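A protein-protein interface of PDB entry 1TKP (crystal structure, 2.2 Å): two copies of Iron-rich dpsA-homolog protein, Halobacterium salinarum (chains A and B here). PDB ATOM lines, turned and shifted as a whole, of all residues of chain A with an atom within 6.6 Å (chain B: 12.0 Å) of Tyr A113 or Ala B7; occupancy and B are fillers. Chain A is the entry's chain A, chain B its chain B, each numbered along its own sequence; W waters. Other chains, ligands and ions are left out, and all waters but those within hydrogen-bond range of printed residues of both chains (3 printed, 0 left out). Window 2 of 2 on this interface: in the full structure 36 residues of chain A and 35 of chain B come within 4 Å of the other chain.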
ATOM      1  N   LYS A  50      -7.966  -9.305  33.825  1.00  0.00           N
ATOM      2  CA  LYS A  50      -6.824  -9.326  32.854  1.00  0.00           C
ATOM      3  C   LYS A  50      -7.422  -9.132  31.422  1.00  0.00           C
ATOM      4  O   LYS A  50      -6.940  -8.294  30.600  1.00  0.00           O
ATOM      5  CB  LYS A  50      -6.119 -10.667  32.920  1.00  0.00           C
ATOM      6  CG  LYS A  50      -5.061 -10.803  31.805  1.00  0.00           C
ATOM      7  CD  LYS A  50      -4.544 -12.173  31.604  1.00  0.00           C
ATOM      8  CE  LYS A  50      -3.158 -12.010  30.810  1.00  0.00           C
ATOM      9  NZ  LYS A  50      -2.413 -13.290  30.869  1.00  0.00           N
ATOM     10  N   HIS A  51      -8.419  -9.950  31.130  1.00  0.00           N
ATOM     11  CA  HIS A  51      -9.021  -9.894  29.832  1.00  0.00           C
ATOM     12  C   HIS A  51      -9.842  -8.621  29.528  1.00  0.00           C
ATOM     13  O   HIS A  51      -9.866  -8.144  28.464  1.00  0.00           O
ATOM     14  CB  HIS A  51      -9.867 -11.131  29.748  1.00  0.00           C
ATOM     15  CG  HIS A  51      -9.036 -12.332  29.771  1.00  0.00           C
ATOM     16  ND1 HIS A  51      -9.554 -13.599  29.889  1.00  0.00           N
ATOM     17  CD2 HIS A  51      -7.692 -12.461  29.595  1.00  0.00           C
ATOM     18  CE1 HIS A  51      -8.567 -14.467  29.815  1.00  0.00           C
ATOM     19  NE2 HIS A  51      -7.421 -13.802  29.654  1.00  0.00           N
ATOM     20  N   ASN A  54      -7.219  -6.108  28.695  1.00  0.00           N
ATOM     21  CA  ASN A  54      -6.379  -6.255  27.499  1.00  0.00           C
ATOM     22  C   ASN A  54      -7.182  -6.437  26.181  1.00  0.00           C
ATOM     23  O   ASN A  54      -6.581  -6.400  25.124  1.00  0.00           O
ATOM     24  CB  ASN A  54      -5.381  -7.398  27.689  1.00  0.00           C
ATOM     25  CG  ASN A  54      -4.232  -7.068  28.654  1.00  0.00           C
ATOM     26  OD1 ASN A  54      -3.355  -6.339  28.307  1.00  0.00           O
ATOM     27  ND2 ASN A  54      -4.134  -7.781  29.738  1.00  0.00           N
ATOM     28  N   GLU A 108      -3.896 -18.578  33.123  1.00  0.00           N
ATOM     29  CA  GLU A 108      -3.036 -18.193  31.986  1.00  0.00           C
ATOM     30  C   GLU A 108      -1.740 -17.674  32.497  1.00  0.00           C
ATOM     31  O   GLU A 108      -1.697 -17.046  33.537  1.00  0.00           O
ATOM     32  CB  GLU A 108      -3.639 -17.037  31.225  1.00  0.00           C
ATOM     33  CG  GLU A 108      -4.597 -17.445  30.127  1.00  0.00           C
ATOM     34  CD  GLU A 108      -5.191 -16.211  29.444  1.00  0.00           C
ATOM     35  OE1 GLU A 108      -6.130 -16.475  28.675  1.00  0.00           O
ATOM     36  OE2 GLU A 108      -4.698 -15.026  29.650  1.00  0.00           O
ATOM     37  N   ASP A 109      -0.664 -17.885  31.771  1.00  0.00           N
ATOM     38  CA  ASP A 109       0.589 -17.271  32.159  1.00  0.00           C
ATOM     39  C   ASP A 109       0.486 -15.781  31.839  1.00  0.00           C
ATOM     40  O   ASP A 109      -0.516 -15.326  31.412  1.00  0.00           O
ATOM     41  CB  ASP A 109       1.734 -17.971  31.498  1.00  0.00           C
ATOM     42  CG  ASP A 109       1.763 -17.821  29.995  1.00  0.00           C
ATOM     43  OD1 ASP A 109       2.486 -18.650  29.356  1.00  0.00           O
ATOM     44  OD2 ASP A 109       1.214 -16.900  29.361  1.00  0.00           O
ATOM     45  N   GLU A 110       1.498 -15.010  32.058  1.00  0.00           N
ATOM     46  CA  GLU A 110       1.411 -13.587  32.042  1.00  0.00           C
ATOM     47  C   GLU A 110       1.394 -12.982  30.611  1.00  0.00           C
ATOM     48  O   GLU A 110       1.117 -11.765  30.403  1.00  0.00           O
ATOM     49  CB  GLU A 110       2.456 -13.032  33.017  1.00  0.00           C
ATOM     50  CG  GLU A 110       1.973 -13.359  34.422  1.00  0.00           C
ATOM     51  CD  GLU A 110       0.678 -12.556  34.803  1.00  0.00           C
ATOM     52  OE1 GLU A 110      -0.296 -13.185  35.318  1.00  0.00           O
ATOM     53  OE2 GLU A 110       0.593 -11.311  34.563  1.00  0.00           O
ATOM     54  N   ASP A 111       1.538 -13.824  29.621  1.00  0.00           N
ATOM     55  CA  ASP A 111       1.343 -13.301  28.297  1.00  0.00           C
ATOM     56  C   ASP A 111      -0.077 -13.000  28.009  1.00  0.00           C
ATOM     57  O   ASP A 111      -1.004 -13.550  28.711  1.00  0.00           O
ATOM     58  CB  ASP A 111       1.905 -14.274  27.321  1.00  0.00           C
ATOM     59  CG  ASP A 111       3.467 -14.307  27.399  1.00  0.00           C
ATOM     60  OD1 ASP A 111       4.050 -13.337  28.012  1.00  0.00           O
ATOM     61  OD2 ASP A 111       4.152 -15.303  27.000  1.00  0.00           O
ATOM     62  N   VAL A 112      -0.310 -12.107  27.016  1.00  0.00           N
ATOM     63  CA  VAL A 112      -1.709 -11.725  26.628  1.00  0.00           C
ATOM     64  C   VAL A 112      -2.104 -12.509  25.413  1.00  0.00           C
ATOM     65  O   VAL A 112      -1.436 -12.486  24.439  1.00  0.00           O
ATOM     66  CB  VAL A 112      -1.761 -10.223  26.283  1.00  0.00           C
ATOM     67  CG1 VAL A 112      -3.186  -9.782  25.873  1.00  0.00           C
ATOM     68  CG2 VAL A 112      -1.067  -9.316  27.437  1.00  0.00           C
ATOM     69  N   TYR A 113      -3.164 -13.252  25.424  1.00  0.00           N
ATOM     70  CA  TYR A 113      -3.509 -13.961  24.211  1.00  0.00           C
ATOM     71  C   TYR A 113      -4.671 -13.278  23.475  1.00  0.00           C
ATOM     72  O   TYR A 113      -5.284 -12.433  24.039  1.00  0.00           O
ATOM     73  CB  TYR A 113      -3.851 -15.353  24.609  1.00  0.00           C
ATOM     74  CG  TYR A 113      -2.674 -16.052  25.266  1.00  0.00           C
ATOM     75  CD1 TYR A 113      -2.555 -16.084  26.673  1.00  0.00           C
ATOM     76  CD2 TYR A 113      -1.657 -16.611  24.497  1.00  0.00           C
ATOM     77  CE1 TYR A 113      -1.513 -16.670  27.292  1.00  0.00           C
ATOM     78  CE2 TYR A 113      -0.604 -17.188  25.104  1.00  0.00           C
ATOM     79  CZ  TYR A 113      -0.539 -17.224  26.497  1.00  0.00           C
ATOM     80  OH  TYR A 113       0.504 -17.835  27.098  1.00  0.00           O
ATOM     81  N   ASP A 114      -5.019 -13.729  22.288  1.00  0.00           N
ATOM     82  CA  ASP A 114      -6.091 -13.177  21.524  1.00  0.00           C
ATOM     83  C   ASP A 114      -7.411 -13.397  22.252  1.00  0.00           C
ATOM     84  O   ASP A 114      -7.421 -14.103  23.253  1.00  0.00           O
ATOM     85  CB  ASP A 114      -6.147 -13.766  20.104  1.00  0.00           C
ATOM     86  CG  ASP A 114      -6.658 -15.201  20.060  1.00  0.00           C
ATOM     87  OD1 ASP A 114      -6.154 -15.967  19.258  1.00  0.00           O
ATOM     88  OD2 ASP A 114      -7.578 -15.664  20.752  1.00  0.00           O
ATOM     89  N   ILE A 115      -8.488 -12.794  21.791  1.00  0.00           N
ATOM     90  CA  ILE A 115      -9.684 -12.737  22.638  1.00  0.00           C
ATOM     91  C   ILE A 115     -10.404 -14.084  22.650  1.00  0.00           C
ATOM     92  O   ILE A 115     -10.882 -14.567  23.752  1.00  0.00           O
ATOM     93  CB  ILE A 115     -10.576 -11.560  22.240  1.00  0.00           C
ATOM     94  CG1 ILE A 115     -11.721 -11.415  23.201  1.00  0.00           C
ATOM     95  CG2 ILE A 115     -10.964 -11.740  20.825  1.00  0.00           C
ATOM     96  CD1 ILE A 115     -11.301 -11.236  24.667  1.00  0.00           C
ATOM     97  N   ARG A 116     -10.443 -14.745  21.489  1.00  0.00           N
ATOM     98  CA  ARG A 116     -10.982 -16.118  21.488  1.00  0.00           C
ATOM     99  C   ARG A 116     -10.244 -17.063  22.455  1.00  0.00           C
ATOM    100  O   ARG A 116     -10.901 -17.818  23.149  1.00  0.00           O
ATOM    101  CB  ARG A 116     -11.072 -16.766  20.120  1.00  0.00           C
ATOM    102  CG  ARG A 116     -11.945 -16.040  19.154  1.00  0.00           C
ATOM    103  CD  ARG A 116     -12.080 -16.826  17.905  1.00  0.00           C
ATOM    104  NE  ARG A 116     -12.708 -18.102  18.263  1.00  0.00           N
ATOM    105  CZ  ARG A 116     -14.008 -18.237  18.334  1.00  0.00           C
ATOM    106  NH1 ARG A 116     -14.831 -17.198  18.087  1.00  0.00           N
ATOM    107  NH2 ARG A 116     -14.496 -19.395  18.661  1.00  0.00           N
ATOM    108  N   THR A 117      -8.899 -16.983  22.553  1.00  0.00           N
ATOM    109  CA  THR A 117      -8.122 -17.889  23.450  1.00  0.00           C
ATOM    110  C   THR A 117      -8.375 -17.493  24.868  1.00  0.00           C
ATOM    111  O   THR A 117      -8.709 -18.293  25.746  1.00  0.00           O
ATOM    112  CB  THR A 117      -6.674 -17.775  23.130  1.00  0.00           C
ATOM    113  OG1 THR A 117      -6.433 -18.238  21.782  1.00  0.00           O
ATOM    114  CG2 THR A 117      -5.783 -18.649  24.086  1.00  0.00           C
ATOM    115  N   SER A 118      -8.426 -16.210  25.098  1.00  0.00           N
ATOM    116  CA  SER A 118      -8.644 -15.728  26.426  1.00  0.00           C
ATOM    117  C   SER A 118     -10.049 -16.158  26.901  1.00  0.00           C
ATOM    118  O   SER A 118     -10.194 -16.647  28.025  1.00  0.00           O
ATOM    119  CB  SER A 118      -8.549 -14.187  26.386  1.00  0.00           C
ATOM    120  OG  SER A 118      -7.259 -13.784  25.955  1.00  0.00           O
ATOM    121  N   ASN A 121     -10.298 -19.944  27.701  1.00  0.00           N
ATOM    122  CA  ASN A 121      -9.675 -20.150  28.968  1.00  0.00           C
ATOM    123  C   ASN A 121     -10.608 -19.674  30.080  1.00  0.00           C
ATOM    124  O   ASN A 121     -10.722 -20.354  31.087  1.00  0.00           O
ATOM    125  CB  ASN A 121      -8.362 -19.330  29.039  1.00  0.00           C
ATOM    126  CG  ASN A 121      -7.285 -19.913  28.215  1.00  0.00           C
ATOM    127  OD1 ASN A 121      -7.439 -20.995  27.810  1.00  0.00           O
ATOM    128  ND2 ASN A 121      -6.176 -19.166  27.908  1.00  0.00           N
ATOM    129  N   ALA B   7       0.790 -15.586  20.866  1.00  0.00           N
ATOM    130  CA  ALA B   7       0.610 -14.547  21.934  1.00  0.00           C
ATOM    131  C   ALA B   7       0.418 -13.127  21.381  1.00  0.00           C
ATOM    132  O   ALA B   7       1.223 -12.632  20.583  1.00  0.00           O
ATOM    133  CB  ALA B   7       1.863 -14.562  22.845  1.00  0.00           C
ATOM    134  N   ARG B   8      -0.573 -12.393  21.810  1.00  0.00           N
ATOM    135  CA  ARG B   8      -0.707 -11.034  21.250  1.00  0.00           C
ATOM    136  C   ARG B   8       0.382 -10.146  21.797  1.00  0.00           C
ATOM    137  O   ARG B   8       0.839  -9.225  21.109  1.00  0.00           O
ATOM    138  CB  ARG B   8      -2.088 -10.358  21.554  1.00  0.00           C
ATOM    139  CG  ARG B   8      -3.017 -10.182  20.365  1.00  0.00           C
ATOM    140  CD  ARG B   8      -4.483  -9.680  20.742  1.00  0.00           C
ATOM    141  NE  ARG B   8      -4.595  -8.273  20.382  1.00  0.00           N
ATOM    142  CZ  ARG B   8      -4.405  -7.917  19.117  1.00  0.00           C
ATOM    143  NH1 ARG B   8      -4.227  -8.878  18.239  1.00  0.00           N
ATOM    144  NH2 ARG B   8      -4.490  -6.654  18.724  1.00  0.00           N
ATOM    145  N   ALA B   9       0.755 -10.371  23.064  1.00  0.00           N
ATOM    146  CA  ALA B   9       1.762  -9.537  23.725  1.00  0.00           C
ATOM    147  C   ALA B   9       2.462 -10.336  24.790  1.00  0.00           C
ATOM    148  O   ALA B   9       1.889 -11.189  25.395  1.00  0.00           O
ATOM    149  CB  ALA B   9       1.227  -8.242  24.336  1.00  0.00           C
ATOM    150  N   THR B  10       3.695  -9.958  25.069  1.00  0.00           N
ATOM    151  CA  THR B  10       4.549 -10.687  25.938  1.00  0.00           C
ATOM    152  C   THR B  10       4.615  -9.891  27.152  1.00  0.00           C
ATOM    153  O   THR B  10       4.787  -8.711  27.053  1.00  0.00           O
ATOM    154  CB  THR B  10       5.932 -10.664  25.209  1.00  0.00           C
ATOM    155  OG1 THR B  10       5.860 -11.651  24.166  1.00  0.00           O
ATOM    156  CG2 THR B  10       7.053 -11.116  26.039  1.00  0.00           C
ATOM    157  N   ALA B  11       4.523 -10.529  28.304  1.00  0.00           N
ATOM    158  CA  ALA B  11       4.663  -9.817  29.571  1.00  0.00           C
ATOM    159  C   ALA B  11       5.904  -9.119  29.462  1.00  0.00           C
ATOM    160  O   ALA B  11       6.905  -9.709  28.996  1.00  0.00           O
ATOM    161  CB  ALA B  11       4.796 -10.760  30.726  1.00  0.00           C
ATOM    162  N   GLY B  12       5.919  -7.899  29.920  1.00  0.00           N
ATOM    163  CA  GLY B  12       7.162  -7.157  29.992  1.00  0.00           C
ATOM    164  C   GLY B  12       7.433  -6.291  28.757  1.00  0.00           C
ATOM    165  O   GLY B  12       8.294  -5.369  28.843  1.00  0.00           O
ATOM    166  N   GLU B  13       6.798  -6.621  27.611  1.00  0.00           N
ATOM    167  CA  GLU B  13       6.873  -5.803  26.368  1.00  0.00           C
ATOM    168  C   GLU B  13       6.083  -4.526  26.570  1.00  0.00           C
ATOM    169  O   GLU B  13       4.976  -4.563  27.129  1.00  0.00           O
ATOM    170  CB  GLU B  13       6.108  -6.456  25.204  1.00  0.00           C
ATOM    171  CG  GLU B  13       6.896  -7.209  24.143  1.00  0.00           C
ATOM    172  CD  GLU B  13       6.037  -7.905  23.048  1.00  0.00           C
ATOM    173  OE1 GLU B  13       6.714  -8.591  22.155  1.00  0.00           O
ATOM    174  OE2 GLU B  13       4.744  -7.775  23.105  1.00  0.00           O
ATOM    175  N   GLU B  15       5.093  -1.235  24.153  1.00  0.00           N
ATOM    176  CA  GLU B  15       5.156  -0.755  22.772  1.00  0.00           C
ATOM    177  C   GLU B  15       4.856   0.729  22.570  1.00  0.00           C
ATOM    178  O   GLU B  15       4.891   1.259  21.436  1.00  0.00           O
ATOM    179  CB  GLU B  15       4.349  -1.682  21.874  1.00  0.00           C
ATOM    180  CG  GLU B  15       2.833  -1.585  21.858  1.00  0.00           C
ATOM    181  CD  GLU B  15       2.176  -2.967  21.591  1.00  0.00           C
ATOM    182  OE1 GLU B  15       2.947  -3.803  20.929  1.00  0.00           O
ATOM    183  OE2 GLU B  15       0.916  -3.208  22.041  1.00  0.00           O
ATOM    184  N   GLN B  86      -1.764  -0.702  30.024  1.00  0.00           N
ATOM    185  CA  GLN B  86      -2.147  -1.271  28.769  1.00  0.00           C
ATOM    186  C   GLN B  86      -2.192  -0.100  27.750  1.00  0.00           C
ATOM    187  O   GLN B  86      -1.808  -0.233  26.571  1.00  0.00           O
ATOM    188  CB  GLN B  86      -3.572  -1.916  28.890  1.00  0.00           C
ATOM    189  CG  GLN B  86      -3.596  -3.296  28.233  1.00  0.00           C
ATOM    190  CD  GLN B  86      -3.971  -3.150  26.770  1.00  0.00           C
ATOM    191  OE1 GLN B  86      -3.814  -4.104  25.925  1.00  0.00           O
ATOM    192  NE2 GLN B  86      -4.386  -1.937  26.433  1.00  0.00           N
ATOM    193  N   GLY B  89       0.884   0.583  26.090  1.00  0.00           N
ATOM    194  CA  GLY B  89       1.423  -0.493  25.302  1.00  0.00           C
ATOM    195  C   GLY B  89       2.085  -1.514  26.161  1.00  0.00           C
ATOM    196  O   GLY B  89       2.873  -2.295  25.667  1.00  0.00           O
ATOM    197  N   GLY B  90       1.799  -1.522  27.453  1.00  0.00           N
ATOM    198  CA  GLY B  90       2.320  -2.519  28.337  1.00  0.00           C
ATOM    199  C   GLY B  90       1.370  -3.631  28.672  1.00  0.00           C
ATOM    200  O   GLY B  90       0.230  -3.696  28.145  1.00  0.00           O
ATOM    201  N   VAL B  91       1.812  -4.507  29.551  1.00  0.00           N
ATOM    202  CA  VAL B  91       1.026  -5.636  29.970  1.00  0.00           C
ATOM    203  C   VAL B  91       0.906  -5.556  31.450  1.00  0.00           C
ATOM    204  O   VAL B  91       1.919  -5.676  32.198  1.00  0.00           O
ATOM    205  CB  VAL B  91       1.681  -6.906  29.654  1.00  0.00           C
ATOM    206  CG1 VAL B  91       0.987  -8.075  30.381  1.00  0.00           C
ATOM    207  CG2 VAL B  91       1.742  -7.153  28.154  1.00  0.00           C
ATOM    208  N   PRO B  92      -0.277  -5.293  31.965  1.00  0.00           N
ATOM    209  CA  PRO B  92      -0.375  -5.209  33.430  1.00  0.00           C
ATOM    210  C   PRO B  92      -0.311  -6.624  34.109  1.00  0.00           C
ATOM    211  O   PRO B  92      -0.882  -7.660  33.666  1.00  0.00           O
ATOM    212  CB  PRO B  92      -1.745  -4.566  33.623  1.00  0.00           C
ATOM    213  CG  PRO B  92      -2.507  -5.103  32.422  1.00  0.00           C
ATOM    214  CD  PRO B  92      -1.562  -5.012  31.249  1.00  0.00           C
ATOM    215  N   ALA B  94      -1.145  -9.670  36.121  1.00  0.00           N
ATOM    216  CA  ALA B  94      -2.495 -10.114  36.178  1.00  0.00           C
ATOM    217  C   ALA B  94      -2.751 -11.229  37.169  1.00  0.00           C
ATOM    218  O   ALA B  94      -3.671 -11.088  37.942  1.00  0.00           O
ATOM    219  CB  ALA B  94      -3.026 -10.498  34.783  1.00  0.00           C
ATOM    220  N   SER B  95      -2.046 -12.375  37.137  1.00  0.00           N
ATOM    221  CA  SER B  95      -2.492 -13.474  38.022  1.00  0.00           C
ATOM    222  C   SER B  95      -2.227 -13.099  39.427  1.00  0.00           C
ATOM    223  O   SER B  95      -1.372 -12.285  39.715  1.00  0.00           O
ATOM    224  CB  SER B  95      -1.801 -14.766  37.742  1.00  0.00           C
ATOM    225  OG  SER B  95      -0.423 -14.598  38.066  1.00  0.00           O
ATOM    226  N   THR B  98       1.468 -13.563  40.270  1.00  0.00           N
ATOM    227  CA  THR B  98       2.298 -12.497  39.704  1.00  0.00           C
ATOM    228  C   THR B  98       2.124 -11.246  40.529  1.00  0.00           C
ATOM    229  O   THR B  98       3.068 -10.538  40.824  1.00  0.00           O
ATOM    230  CB  THR B  98       1.789 -12.254  38.246  1.00  0.00           C
ATOM    231  OG1 THR B  98       1.882 -13.474  37.494  1.00  0.00           O
ATOM    232  CG2 THR B  98       2.547 -11.272  37.539  1.00  0.00           C
HETATM  233  O   HOH W   1      -4.815  -7.298  23.488  1.00  0.00           O
HETATM  234  O   HOH W   2      -2.112  -8.398  31.513  1.00  0.00           O
HETATM  235  O   HOH W   3      -0.651 -10.728  32.318  1.00  0.00           O
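N of Ala B11 lies within hydrogen-bond range of OD1 of Asp A111 (2.9 Å).
OG1 of Thr B98 sits close to OE1 of Glu A110, 3.1 Å away.
The backbone NH (N) of Ser B95 sits at hydrogen-bond distance from the side-chain carboxylate (OE1) of Glu A110 (2.7 Å).
The side-chain amide oxygen (OE1) of Gln B86 lies close to the side-chain amide oxygen (OD1) of Asn A54, at 3.3 Å.
The backbone NH of Val A112 is in hydrogen-bond range of the backbone carbonyl oxygen of Ala B9, at 2.9 Å.
The backbone NH (N) of Arg B8 sits at hydrogen-bond distance from the backbone carbonyl oxygen (O) of Val A112 (2.8 Å).
N of Ala B94 sits at hydrogen-bond distance from OE2 of Glu A110.
The backbone carbonyl oxygen (O) of Asp A111 is in hydrogen-bond range of the side-chain amino group (NZ) of Lys A50.
N of Thr B10 lies within hydrogen-bond range of OE2 of Glu B13 (3.1 Å).
The backbone carbonyl oxygen of Lys A50 lies within hydrogen-bond range of the side-chain amide nitrogen of Asn A54.
The backbone carbonyl oxygen of Tyr A113 lies within hydrogen-bond range of the side-chain hydroxyl of Ser A118, at 3.1 Å.
OE2 of Glu A108 is in salt-bridge range of NZ of Lys A50 (3.1 Å).
N of Asp A111 lies within hydrogen-bond range of OD2 of Asp A109 (3.1 Å).
CB of Lys A50 touches CB of Ala B94 (3.6 Å).
OD1 of Asn A54 touches CD of Pro B92, at 3.7 Å.
Ala B11 touches Glu A110.
O of Glu A110 touches CG1 of Val B91, at 3.7 Å.
Ala B9 touches Asp A111 (O to CA, 3.6 Å).
Asp A111 touches Thr B10 (OD1 to CA, 3.4 Å).
Ala B7 touches Val A112 (C to O, 3.6 Å).
CG2 of Val B91 touches CG2 of Val A112 (3.6 Å).
CD2 of Tyr A113 touches CA of Ala B7, 3.996 Å away.
Asp A114 touches Arg B8.
Of the printed residues of chain B, Tyr A113 touches Ala B7.
Of the printed residues of chain A, Ala B7 touches Val A112 (3.6 Å) and Tyr A113 (3.996 Å).
No residue of chain B comes within 4 Å of Glu A108.
No residue of chain B comes within 4 Å of Asp A109.
Asp A111 touches just these residues of chain B: Ala B9 (3.6 Å), Thr B10 (3.4 Å) and Ala B11 (2.9 Å).
Of the printed residues of chain B, Asp A114 touches Arg B8 (3.9 Å).
No residue of chain B comes within 4 Å of Thr A117.
No residue of chain B comes within 4 Å of Ser A118.
Of the printed residues of chain A, Pro B92 touches Asn A54.
Of the printed residues of chain B, Asn A54 touches Gln B86 (3.1 Å) and Pro B92 (3.7 Å).
Printed residues of chain B within 4 Å of Glu A110: Ala B11 (3.8 Å), Val B91 (3.7 Å), Ala B94 (2.9 Å), Ser B95 (2.7 Å) and Thr B98 (3.1 Å).
Gly B89 touches none of the printed residues of chain A.
Gly B90 touches none of the printed residues of chain A.
Of the 16 printed residues of chain B, 11 touch a printed residue of chain A.
Along chain B the printed residues that touch a printed residue of chain A span positions 7 to 98.
Of the 15 printed residues of chain A, 7 touch a printed residue of chain B.
Hydrophobic or aromatic side chains of chain A that line the printed part of chain B: Val A112 and Tyr A113.
No position is printed for both chains.
Water W1 bridges O of Asn A54 (2.6 Å) and NE of Arg B8 (3.3 Å).
Water W2 bridges the backbone carbonyl oxygen (O) of Pro B92 (2.6 Å) and the side-chain amide nitrogen (ND2) of Asn A54 (2.8 Å).
Water W3 lies within hydrogen-bond range of OE2 of Glu A110 (2.6 Å), O of Pro B92 (3.4 Å) and NZ of Lys A50 (3.4 Å).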
